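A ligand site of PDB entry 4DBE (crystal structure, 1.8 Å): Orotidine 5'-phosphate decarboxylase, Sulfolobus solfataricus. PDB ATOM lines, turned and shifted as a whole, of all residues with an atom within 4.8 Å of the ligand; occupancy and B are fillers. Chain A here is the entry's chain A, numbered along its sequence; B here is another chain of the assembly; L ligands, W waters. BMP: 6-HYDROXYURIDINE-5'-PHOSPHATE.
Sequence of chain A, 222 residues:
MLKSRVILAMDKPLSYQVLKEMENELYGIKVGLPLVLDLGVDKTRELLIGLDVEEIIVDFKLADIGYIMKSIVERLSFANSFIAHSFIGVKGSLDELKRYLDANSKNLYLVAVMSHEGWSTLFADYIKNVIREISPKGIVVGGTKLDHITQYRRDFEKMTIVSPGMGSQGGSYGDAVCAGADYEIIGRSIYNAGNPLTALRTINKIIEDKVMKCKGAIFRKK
N of Arg 188 is in hydrogen-bond range of OP2 of the ligand (2.6 Å). The guanidinium group (NE) of Arg 188 is in salt-bridge range of an oxygen (OP2) of the ligand, 2.7 Å away. The side-chain amino group of Lys 61 sits at hydrogen-bond distance from an oxygen (O1) of the ligand, 2.6 Å away. OD1 of Asp 64 of chain B lies within hydrogen-bond range of O2' of the ligand (2.6 Å). N of Gly 187 lies within hydrogen-bond range of OP3 of the ligand (2.7 Å). OD2 of Asp 11 sits at hydrogen-bond distance from O3' of the ligand, at 2.7 Å. N of Ser 115 sits at hydrogen-bond distance from O4 of the ligand (2.8 Å). The side-chain hydroxyl of Ser 115 sits at hydrogen-bond distance from a nitrogen (N3) of the ligand (2.7 Å). The side-chain amino group (NZ) of Lys 30 sits at hydrogen-bond distance from an oxygen (O3') of the ligand, 2.8 Å away. NE2 of Gln 169 is in hydrogen-bond range of OP1 of the ligand, 2.9 Å away.
The side-chain hydroxyl (OG) of Ser 168 lies close to the guanidinium group (NH1) of Arg 188. The side-chain amino group (NZ) of Lys 61 is in salt-bridge range of the side-chain carboxylate (OD2) of Asp 64 of chain B (2.9 Å). NZ of Lys 61 lies within salt-bridge range of OD2 of Asp 59, at 2.6 Å. OG of Ser 115 sits at hydrogen-bond distance from OE1 of Gln 169, 2.6 Å away. NZ of Lys 30 is in salt-bridge range of OD2 of Asp 59. N of Ala 9 lies within hydrogen-bond range of O of Ile 186 (2.8 Å).
Merely in contact with the ligand: Ala 9, Asp 59, Met 114, Pro 164, Met 166, Ile 185, Ile 186, Ile 65 of chain B and Ile 68 of chain B. The nearest printed residue that does not touch the ligand is Val 140 (4.01 Å).
Water W2 lies within hydrogen-bond range of OP1 of the ligand (2.6 Å), O of Met 166 (2.8 Å), N of Gln 169 (2.9 Å) and N of Ser 168 (3.5 Å). Water W4 lies within hydrogen-bond range of the backbone carbonyl oxygen of Ile 185, an oxygen (OP3) of the ligand, the backbone NH of Gly 165 and the backbone NH of Met 166. Water W5 lies within hydrogen-bond range of the side-chain hydroxyl (OH) of Tyr 191 (2.6 Å), the side-chain carboxylate (OD2) of Asp 11 (2.7 Å) and an oxygen (OP2) of the ligand (2.9 Å). Water W3 lies within hydrogen-bond range of the side-chain carboxylate (OD1) of Asp 11 (2.9 Å), an oxygen (O3') of the ligand (2.9 Å) and the side-chain amino group (NZ) of Lys 30 (3.2 Å).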
ATOM      1  N   ALA A   9      12.977  -5.211   2.727  1.00  0.00           N
ATOM      2  CA  ALA A   9      13.729  -6.332   3.246  1.00  0.00           C
ATOM      3  C   ALA A   9      13.394  -6.452   4.736  1.00  0.00           C
ATOM      4  O   ALA A   9      14.007  -5.787   5.573  1.00  0.00           O
ATOM      5  CB  ALA A   9      15.228  -6.172   3.032  1.00  0.00           C
ATOM      6  N   ASP A  11      14.004  -7.928   7.593  1.00  0.00           N
ATOM      7  CA  ASP A  11      14.979  -8.729   8.309  1.00  0.00           C
ATOM      8  C   ASP A  11      14.820  -8.562   9.815  1.00  0.00           C
ATOM      9  O   ASP A  11      15.552  -9.151  10.595  1.00  0.00           O
ATOM     10  CB  ASP A  11      16.388  -8.309   7.884  1.00  0.00           C
ATOM     11  CG  ASP A  11      16.657  -8.637   6.439  1.00  0.00           C
ATOM     12  OD1 ASP A  11      16.245  -9.740   6.005  1.00  0.00           O
ATOM     13  OD2 ASP A  11      17.280  -7.802   5.730  1.00  0.00           O
ATOM     14  N   LYS A  30      10.465  -8.816   1.149  1.00  0.00           N
ATOM     15  CA  LYS A  30      11.412  -9.926   1.170  1.00  0.00           C
ATOM     16  C   LYS A  30      11.558 -10.377   2.634  1.00  0.00           C
ATOM     17  O   LYS A  30      12.031  -9.626   3.487  1.00  0.00           O
ATOM     18  CB  LYS A  30      12.753  -9.504   0.587  1.00  0.00           C
ATOM     19  CG  LYS A  30      13.725 -10.654   0.384  1.00  0.00           C
ATOM     20  CD  LYS A  30      15.006 -10.187  -0.325  1.00  0.00           C
ATOM     21  CE  LYS A  30      15.964  -9.441   0.598  1.00  0.00           C
ATOM     22  NZ  LYS A  30      16.468 -10.299   1.731  1.00  0.00           N
ATOM     23  N   ASP A  59      13.555 -15.195   1.486  1.00  0.00           N
ATOM     24  CA  ASP A  59      14.979 -15.171   1.172  1.00  0.00           C
ATOM     25  C   ASP A  59      15.819 -15.800   2.269  1.00  0.00           C
ATOM     26  O   ASP A  59      16.229 -15.119   3.224  1.00  0.00           O
ATOM     27  CB  ASP A  59      15.469 -13.739   0.875  1.00  0.00           C
ATOM     28  CG  ASP A  59      16.969 -13.685   0.571  1.00  0.00           C
ATOM     29  OD1 ASP A  59      17.573 -14.749   0.367  1.00  0.00           O
ATOM     30  OD2 ASP A  59      17.547 -12.579   0.535  1.00  0.00           O
ATOM     31  N   LYS A  61      18.529 -17.406   1.100  1.00  0.00           N
ATOM     32  CA  LYS A  61      19.791 -17.556   0.357  1.00  0.00           C
ATOM     33  C   LYS A  61      20.110 -19.037   0.124  1.00  0.00           C
ATOM     34  O   LYS A  61      21.247 -19.497   0.357  1.00  0.00           O
ATOM     35  CB  LYS A  61      20.946 -16.876   1.118  1.00  0.00           C
ATOM     36  CG  LYS A  61      20.899 -15.348   1.172  1.00  0.00           C
ATOM     37  CD  LYS A  61      20.886 -14.714  -0.233  1.00  0.00           C
ATOM     38  CE  LYS A  61      21.143 -13.209  -0.165  1.00  0.00           C
ATOM     39  NZ  LYS A  61      20.124 -12.463   0.652  1.00  0.00           N
ATOM     40  N   VAL A 113      24.855 -11.272  -8.731  1.00  0.00           N
ATOM     41  CA  VAL A 113      26.001 -10.484  -8.285  1.00  0.00           C
ATOM     42  C   VAL A 113      25.639  -9.882  -6.938  1.00  0.00           C
ATOM     43  O   VAL A 113      24.613  -9.208  -6.810  1.00  0.00           O
ATOM     44  CB  VAL A 113      26.283  -9.348  -9.267  1.00  0.00           C
ATOM     45  CG1 VAL A 113      27.495  -8.515  -8.781  1.00  0.00           C
ATOM     46  CG2 VAL A 113      26.491  -9.894 -10.687  1.00  0.00           C
ATOM     47  N   MET A 114      26.457 -10.112  -5.920  1.00  0.00           N
ATOM     48  CA  MET A 114      26.122  -9.581  -4.603  1.00  0.00           C
ATOM     49  C   MET A 114      26.599  -8.134  -4.396  1.00  0.00           C
ATOM     50  O   MET A 114      27.360  -7.594  -5.216  1.00  0.00           O
ATOM     51  CB  MET A 114      26.571 -10.516  -3.478  1.00  0.00           C
ATOM     52  CG  MET A 114      25.755 -11.799  -3.418  1.00  0.00           C
ATOM     53  SD  MET A 114      26.162 -12.793  -1.980  1.00  0.00           S
ATOM     54  CE  MET A 114      25.455 -11.807  -0.665  1.00  0.00           C
ATOM     55  N   SER A 115      26.138  -7.520  -3.310  1.00  0.00           N
ATOM     56  CA  SER A 115      26.353  -6.084  -3.108  1.00  0.00           C
ATOM     57  C   SER A 115      27.654  -5.732  -2.387  1.00  0.00           C
ATOM     58  O   SER A 115      28.132  -4.609  -2.491  1.00  0.00           O
ATOM     59  CB  SER A 115      25.157  -5.462  -2.385  1.00  0.00           C
ATOM     60  OG  SER A 115      24.983  -6.038  -1.103  1.00  0.00           O
ATOM     61  N   VAL A 140      19.078 -11.498  -8.581  1.00  0.00           N
ATOM     62  CA  VAL A 140      19.487 -10.459  -7.661  1.00  0.00           C
ATOM     63  C   VAL A 140      20.836  -9.925  -8.122  1.00  0.00           C
ATOM     64  O   VAL A 140      21.783 -10.698  -8.290  1.00  0.00           O
ATOM     65  CB  VAL A 140      19.631 -10.990  -6.200  1.00  0.00           C
ATOM     66  CG1 VAL A 140      19.819  -9.823  -5.214  1.00  0.00           C
ATOM     67  CG2 VAL A 140      18.424 -11.855  -5.796  1.00  0.00           C
ATOM     68  N   PRO A 164      19.530  -5.027  -4.139  1.00  0.00           N
ATOM     69  CA  PRO A 164      19.725  -4.580  -2.755  1.00  0.00           C
ATOM     70  C   PRO A 164      21.033  -3.783  -2.615  1.00  0.00           C
ATOM     71  O   PRO A 164      21.803  -3.724  -3.574  1.00  0.00           O
ATOM     72  CB  PRO A 164      19.836  -5.900  -1.997  1.00  0.00           C
ATOM     73  CG  PRO A 164      20.545  -6.797  -2.976  1.00  0.00           C
ATOM     74  CD  PRO A 164      20.131  -6.349  -4.374  1.00  0.00           C
ATOM     75  N   GLY A 165      21.264  -3.185  -1.445  1.00  0.00           N
ATOM     76  CA  GLY A 165      22.474  -2.398  -1.192  1.00  0.00           C
ATOM     77  C   GLY A 165      22.183  -0.915  -1.258  1.00  0.00           C
ATOM     78  O   GLY A 165      23.111  -0.085  -1.387  1.00  0.00           O
ATOM     79  N   MET A 166      20.899  -0.578  -1.187  1.00  0.00           N
ATOM     80  CA  MET A 166      20.476   0.818  -1.232  1.00  0.00           C
ATOM     81  C   MET A 166      20.311   1.420   0.171  1.00  0.00           C
ATOM     82  O   MET A 166      19.773   0.789   1.093  1.00  0.00           O
ATOM     83  CB  MET A 166      19.171   0.978  -2.015  1.00  0.00           C
ATOM     84  CG  MET A 166      19.125   0.184  -3.333  1.00  0.00           C
ATOM     85  SD  MET A 166      20.570   0.349  -4.401  1.00  0.00           S
ATOM     86  CE  MET A 166      20.328   1.983  -5.133  1.00  0.00           C
ATOM     87  N   SER A 168      21.766   2.017   3.411  1.00  0.00           N
ATOM     88  CA  SER A 168      22.800   1.596   4.345  1.00  0.00           C
ATOM     89  C   SER A 168      24.117   1.227   3.670  1.00  0.00           C
ATOM     90  O   SER A 168      25.188   1.666   4.103  1.00  0.00           O
ATOM     91  CB  SER A 168      22.297   0.419   5.200  1.00  0.00           C
ATOM     92  OG  SER A 168      23.266   0.055   6.160  1.00  0.00           O
ATOM     93  N   GLN A 169      24.041   0.426   2.611  1.00  0.00           N
ATOM     94  CA  GLN A 169      25.250  -0.068   1.963  1.00  0.00           C
ATOM     95  C   GLN A 169      25.894   0.898   0.963  1.00  0.00           C
ATOM     96  O   GLN A 169      26.996   0.642   0.501  1.00  0.00           O
ATOM     97  CB  GLN A 169      24.992  -1.417   1.278  1.00  0.00           C
ATOM     98  CG  GLN A 169      24.770  -2.568   2.283  1.00  0.00           C
ATOM     99  CD  GLN A 169      24.460  -3.879   1.569  1.00  0.00           C
ATOM    100  OE1 GLN A 169      25.321  -4.459   0.909  1.00  0.00           O
ATOM    101  NE2 GLN A 169      23.230  -4.361   1.727  1.00  0.00           N
ATOM    102  N   ILE A 185      15.701  -3.427  -3.360  1.00  0.00           N
ATOM    103  CA  ILE A 185      15.467  -4.057  -2.076  1.00  0.00           C
ATOM    104  C   ILE A 185      16.049  -3.169  -0.993  1.00  0.00           C
ATOM    105  O   ILE A 185      17.232  -2.812  -1.049  1.00  0.00           O
ATOM    106  CB  ILE A 185      16.175  -5.408  -2.019  1.00  0.00           C
ATOM    107  CG1 ILE A 185      15.546  -6.380  -3.014  1.00  0.00           C
ATOM    108  CG2 ILE A 185      16.096  -5.991  -0.598  1.00  0.00           C
ATOM    109  CD1 ILE A 185      16.404  -7.619  -3.297  1.00  0.00           C
ATOM    110  N   ILE A 186      15.240  -2.810   0.003  1.00  0.00           N
ATOM    111  CA  ILE A 186      15.708  -1.864   1.021  1.00  0.00           C
ATOM    112  C   ILE A 186      15.323  -2.346   2.415  1.00  0.00           C
ATOM    113  O   ILE A 186      14.135  -2.610   2.686  1.00  0.00           O
ATOM    114  CB  ILE A 186      15.125  -0.459   0.769  1.00  0.00           C
ATOM    115  CG1 ILE A 186      15.450   0.003  -0.648  1.00  0.00           C
ATOM    116  CG2 ILE A 186      15.641   0.541   1.801  1.00  0.00           C
ATOM    117  CD1 ILE A 186      14.638   1.204  -1.087  1.00  0.00           C
ATOM    118  N   GLY A 187      16.319  -2.454   3.296  1.00  0.00           N
ATOM    119  CA  GLY A 187      16.092  -2.981   4.638  1.00  0.00           C
ATOM    120  C   GLY A 187      16.234  -1.911   5.715  1.00  0.00           C
ATOM    121  O   GLY A 187      15.281  -1.179   6.019  1.00  0.00           O
ATOM    122  N   ARG A 188      17.422  -1.818   6.277  1.00  0.00           N
ATOM    123  CA  ARG A 188      17.680  -0.914   7.421  1.00  0.00           C
ATOM    124  C   ARG A 188      17.241   0.542   7.248  1.00  0.00           C
ATOM    125  O   ARG A 188      16.807   1.167   8.215  1.00  0.00           O
ATOM    126  CB  ARG A 188      19.164  -0.974   7.797  1.00  0.00           C
ATOM    127  CG  ARG A 188      19.561  -2.235   8.504  1.00  0.00           C
ATOM    128  CD  ARG A 188      21.065  -2.409   8.496  1.00  0.00           C
ATOM    129  NE  ARG A 188      21.571  -2.786   7.178  1.00  0.00           N
ATOM    130  CZ  ARG A 188      22.852  -2.989   6.926  1.00  0.00           C
ATOM    131  NH1 ARG A 188      23.761  -2.812   7.882  1.00  0.00           N
ATOM    132  NH2 ARG A 188      23.248  -3.342   5.712  1.00  0.00           N
ATOM    133  N   SER A 189      17.367   1.097   6.044  1.00  0.00           N
ATOM    134  CA  SER A 189      17.044   2.506   5.848  1.00  0.00           C
ATOM    135  C   SER A 189      15.552   2.745   6.059  1.00  0.00           C
ATOM    136  O   SER A 189      15.135   3.875   6.287  1.00  0.00           O
ATOM    137  CB  SER A 189      17.452   2.992   4.447  1.00  0.00           C
ATOM    138  OG  SER A 189      18.848   3.070   4.355  1.00  0.00           O
ATOM    139  N   TYR A 191      13.415   0.047   8.021  1.00  0.00           N
ATOM    140  CA  TYR A 191      12.950  -0.539   9.298  1.00  0.00           C
ATOM    141  C   TYR A 191      13.628  -0.035  10.571  1.00  0.00           C
ATOM    142  O   TYR A 191      13.073  -0.147  11.664  1.00  0.00           O
ATOM    143  CB  TYR A 191      12.893  -2.077   9.249  1.00  0.00           C
ATOM    144  CG  TYR A 191      14.218  -2.816   9.155  1.00  0.00           C
ATOM    145  CD1 TYR A 191      15.167  -2.747  10.181  1.00  0.00           C
ATOM    146  CD2 TYR A 191      14.497  -3.646   8.061  1.00  0.00           C
ATOM    147  CE1 TYR A 191      16.364  -3.463  10.099  1.00  0.00           C
ATOM    148  CE2 TYR A 191      15.704  -4.354   7.975  1.00  0.00           C
ATOM    149  CZ  TYR A 191      16.621  -4.268   9.000  1.00  0.00           C
ATOM    150  OH  TYR A 191      17.805  -4.980   8.921  1.00  0.00           O
ATOM    151  N   ASP B  64      25.456 -14.515   2.897  1.00  0.00           N
ATOM    152  CA  ASP B  64      24.805 -13.233   2.795  1.00  0.00           C
ATOM    153  C   ASP B  64      25.842 -12.166   3.091  1.00  0.00           C
ATOM    154  O   ASP B  64      27.028 -12.473   3.211  1.00  0.00           O
ATOM    155  CB  ASP B  64      23.659 -13.151   3.798  1.00  0.00           C
ATOM    156  CG  ASP B  64      22.515 -12.299   3.306  1.00  0.00           C
ATOM    157  OD1 ASP B  64      22.741 -11.135   2.935  1.00  0.00           O
ATOM    158  OD2 ASP B  64      21.370 -12.811   3.289  1.00  0.00           O
ATOM    159  N   ILE B  65      25.404 -10.924   3.212  1.00  0.00           N
ATOM    160  CA  ILE B  65      26.306  -9.873   3.682  1.00  0.00           C
ATOM    161  C   ILE B  65      26.605 -10.111   5.169  1.00  0.00           C
ATOM    162  O   ILE B  65      25.888 -10.879   5.855  1.00  0.00           O
ATOM    163  CB  ILE B  65      25.732  -8.465   3.439  1.00  0.00           C
ATOM    164  CG1 ILE B  65      24.414  -8.272   4.201  1.00  0.00           C
ATOM    165  CG2 ILE B  65      25.567  -8.212   1.931  1.00  0.00           C
ATOM    166  CD1 ILE B  65      23.858  -6.846   4.126  1.00  0.00           C
ATOM    167  N   TYR B  67      26.337  -8.293   7.877  1.00  0.00           N
ATOM    168  CA  TYR B  67      25.327  -7.854   8.827  1.00  0.00           C
ATOM    169  C   TYR B  67      24.257  -8.922   9.044  1.00  0.00           C
ATOM    170  O   TYR B  67      23.874  -9.216  10.172  1.00  0.00           O
ATOM    171  CB  TYR B  67      24.694  -6.554   8.341  1.00  0.00           C
ATOM    172  CG  TYR B  67      23.379  -6.199   9.017  1.00  0.00           C
ATOM    173  CD1 TYR B  67      23.335  -5.844  10.361  1.00  0.00           C
ATOM    174  CD2 TYR B  67      22.196  -6.210   8.305  1.00  0.00           C
ATOM    175  CE1 TYR B  67      22.135  -5.520  10.976  1.00  0.00           C
ATOM    176  CE2 TYR B  67      20.995  -5.902   8.906  1.00  0.00           C
ATOM    177  CZ  TYR B  67      20.969  -5.553  10.239  1.00  0.00           C
ATOM    178  OH  TYR B  67      19.759  -5.226  10.833  1.00  0.00           O
ATOM    179  N   ILE B  68      23.796  -9.508   7.945  1.00  0.00           N
ATOM    180  CA  ILE B  68      22.747 -10.522   8.000  1.00  0.00           C
ATOM    181  C   ILE B  68      23.269 -11.840   8.550  1.00  0.00           C
ATOM    182  O   ILE B  68      22.624 -12.467   9.385  1.00  0.00           O
ATOM    183  CB  ILE B  68      22.105 -10.710   6.604  1.00  0.00           C
ATOM    184  CG1 ILE B  68      21.326  -9.447   6.206  1.00  0.00           C
ATOM    185  CG2 ILE B  68      21.186 -11.927   6.595  1.00  0.00           C
ATOM    186  CD1 ILE B  68      20.059  -9.200   7.036  1.00  0.00           C
HETATM  187  P   BMP L   1      19.900  -3.351   3.919  1.00  0.00           P
HETATM  188  OP1 BMP L   1      21.294  -3.137   3.492  1.00  0.00           O
HETATM  189  OP2 BMP L   1      19.516  -3.067   5.463  1.00  0.00           O
HETATM  190  OP3 BMP L   1      18.984  -2.361   3.073  1.00  0.00           O
HETATM  191  O5' BMP L   1      19.407  -4.820   3.519  1.00  0.00           O
HETATM  192  C5' BMP L   1      19.719  -5.403   2.273  1.00  0.00           C
HETATM  193  C4' BMP L   1      18.948  -6.693   2.061  1.00  0.00           C
HETATM  194  O4' BMP L   1      19.325  -7.275   0.791  1.00  0.00           O
HETATM  195  C3' BMP L   1      19.209  -7.771   3.123  1.00  0.00           C
HETATM  196  O3' BMP L   1      18.046  -8.582   3.281  1.00  0.00           O
HETATM  197  C2' BMP L   1      20.311  -8.603   2.475  1.00  0.00           C
HETATM  198  O2' BMP L   1      20.382  -9.935   2.931  1.00  0.00           O
HETATM  199  C1' BMP L   1      19.905  -8.550   0.990  1.00  0.00           C
HETATM  200  N1  BMP L   1      21.036  -8.699   0.051  1.00  0.00           N
HETATM  201  C2  BMP L   1      22.117  -7.888   0.110  1.00  0.00           C
HETATM  202  O2  BMP L   1      22.216  -7.024   0.957  1.00  0.00           O
HETATM  203  N3  BMP L   1      23.140  -8.047  -0.762  1.00  0.00           N
HETATM  204  C4  BMP L   1      23.093  -8.991  -1.735  1.00  0.00           C
HETATM  205  O4  BMP L   1      24.027  -9.104  -2.525  1.00  0.00           O
HETATM  206  C5  BMP L   1      21.965  -9.823  -1.832  1.00  0.00           C
HETATM  207  C6  BMP L   1      20.938  -9.653  -0.925  1.00  0.00           C
HETATM  208  O1  BMP L   1      19.843 -10.416  -0.995  1.00  0.00           O
HETATM  209  O   HOH W   1      18.908   0.121   3.847  1.00  0.00           O
HETATM  210  O   HOH W   2      21.731  -1.107   1.898  1.00  0.00           O
HETATM  211  O   HOH W   3      18.019 -11.323   4.324  1.00  0.00           O
HETATM  212  O   HOH W   4      19.323  -2.568   0.451  1.00  0.00           O
HETATM  213  O   HOH W   5      18.564  -5.610   6.519  1.00  0.00           O
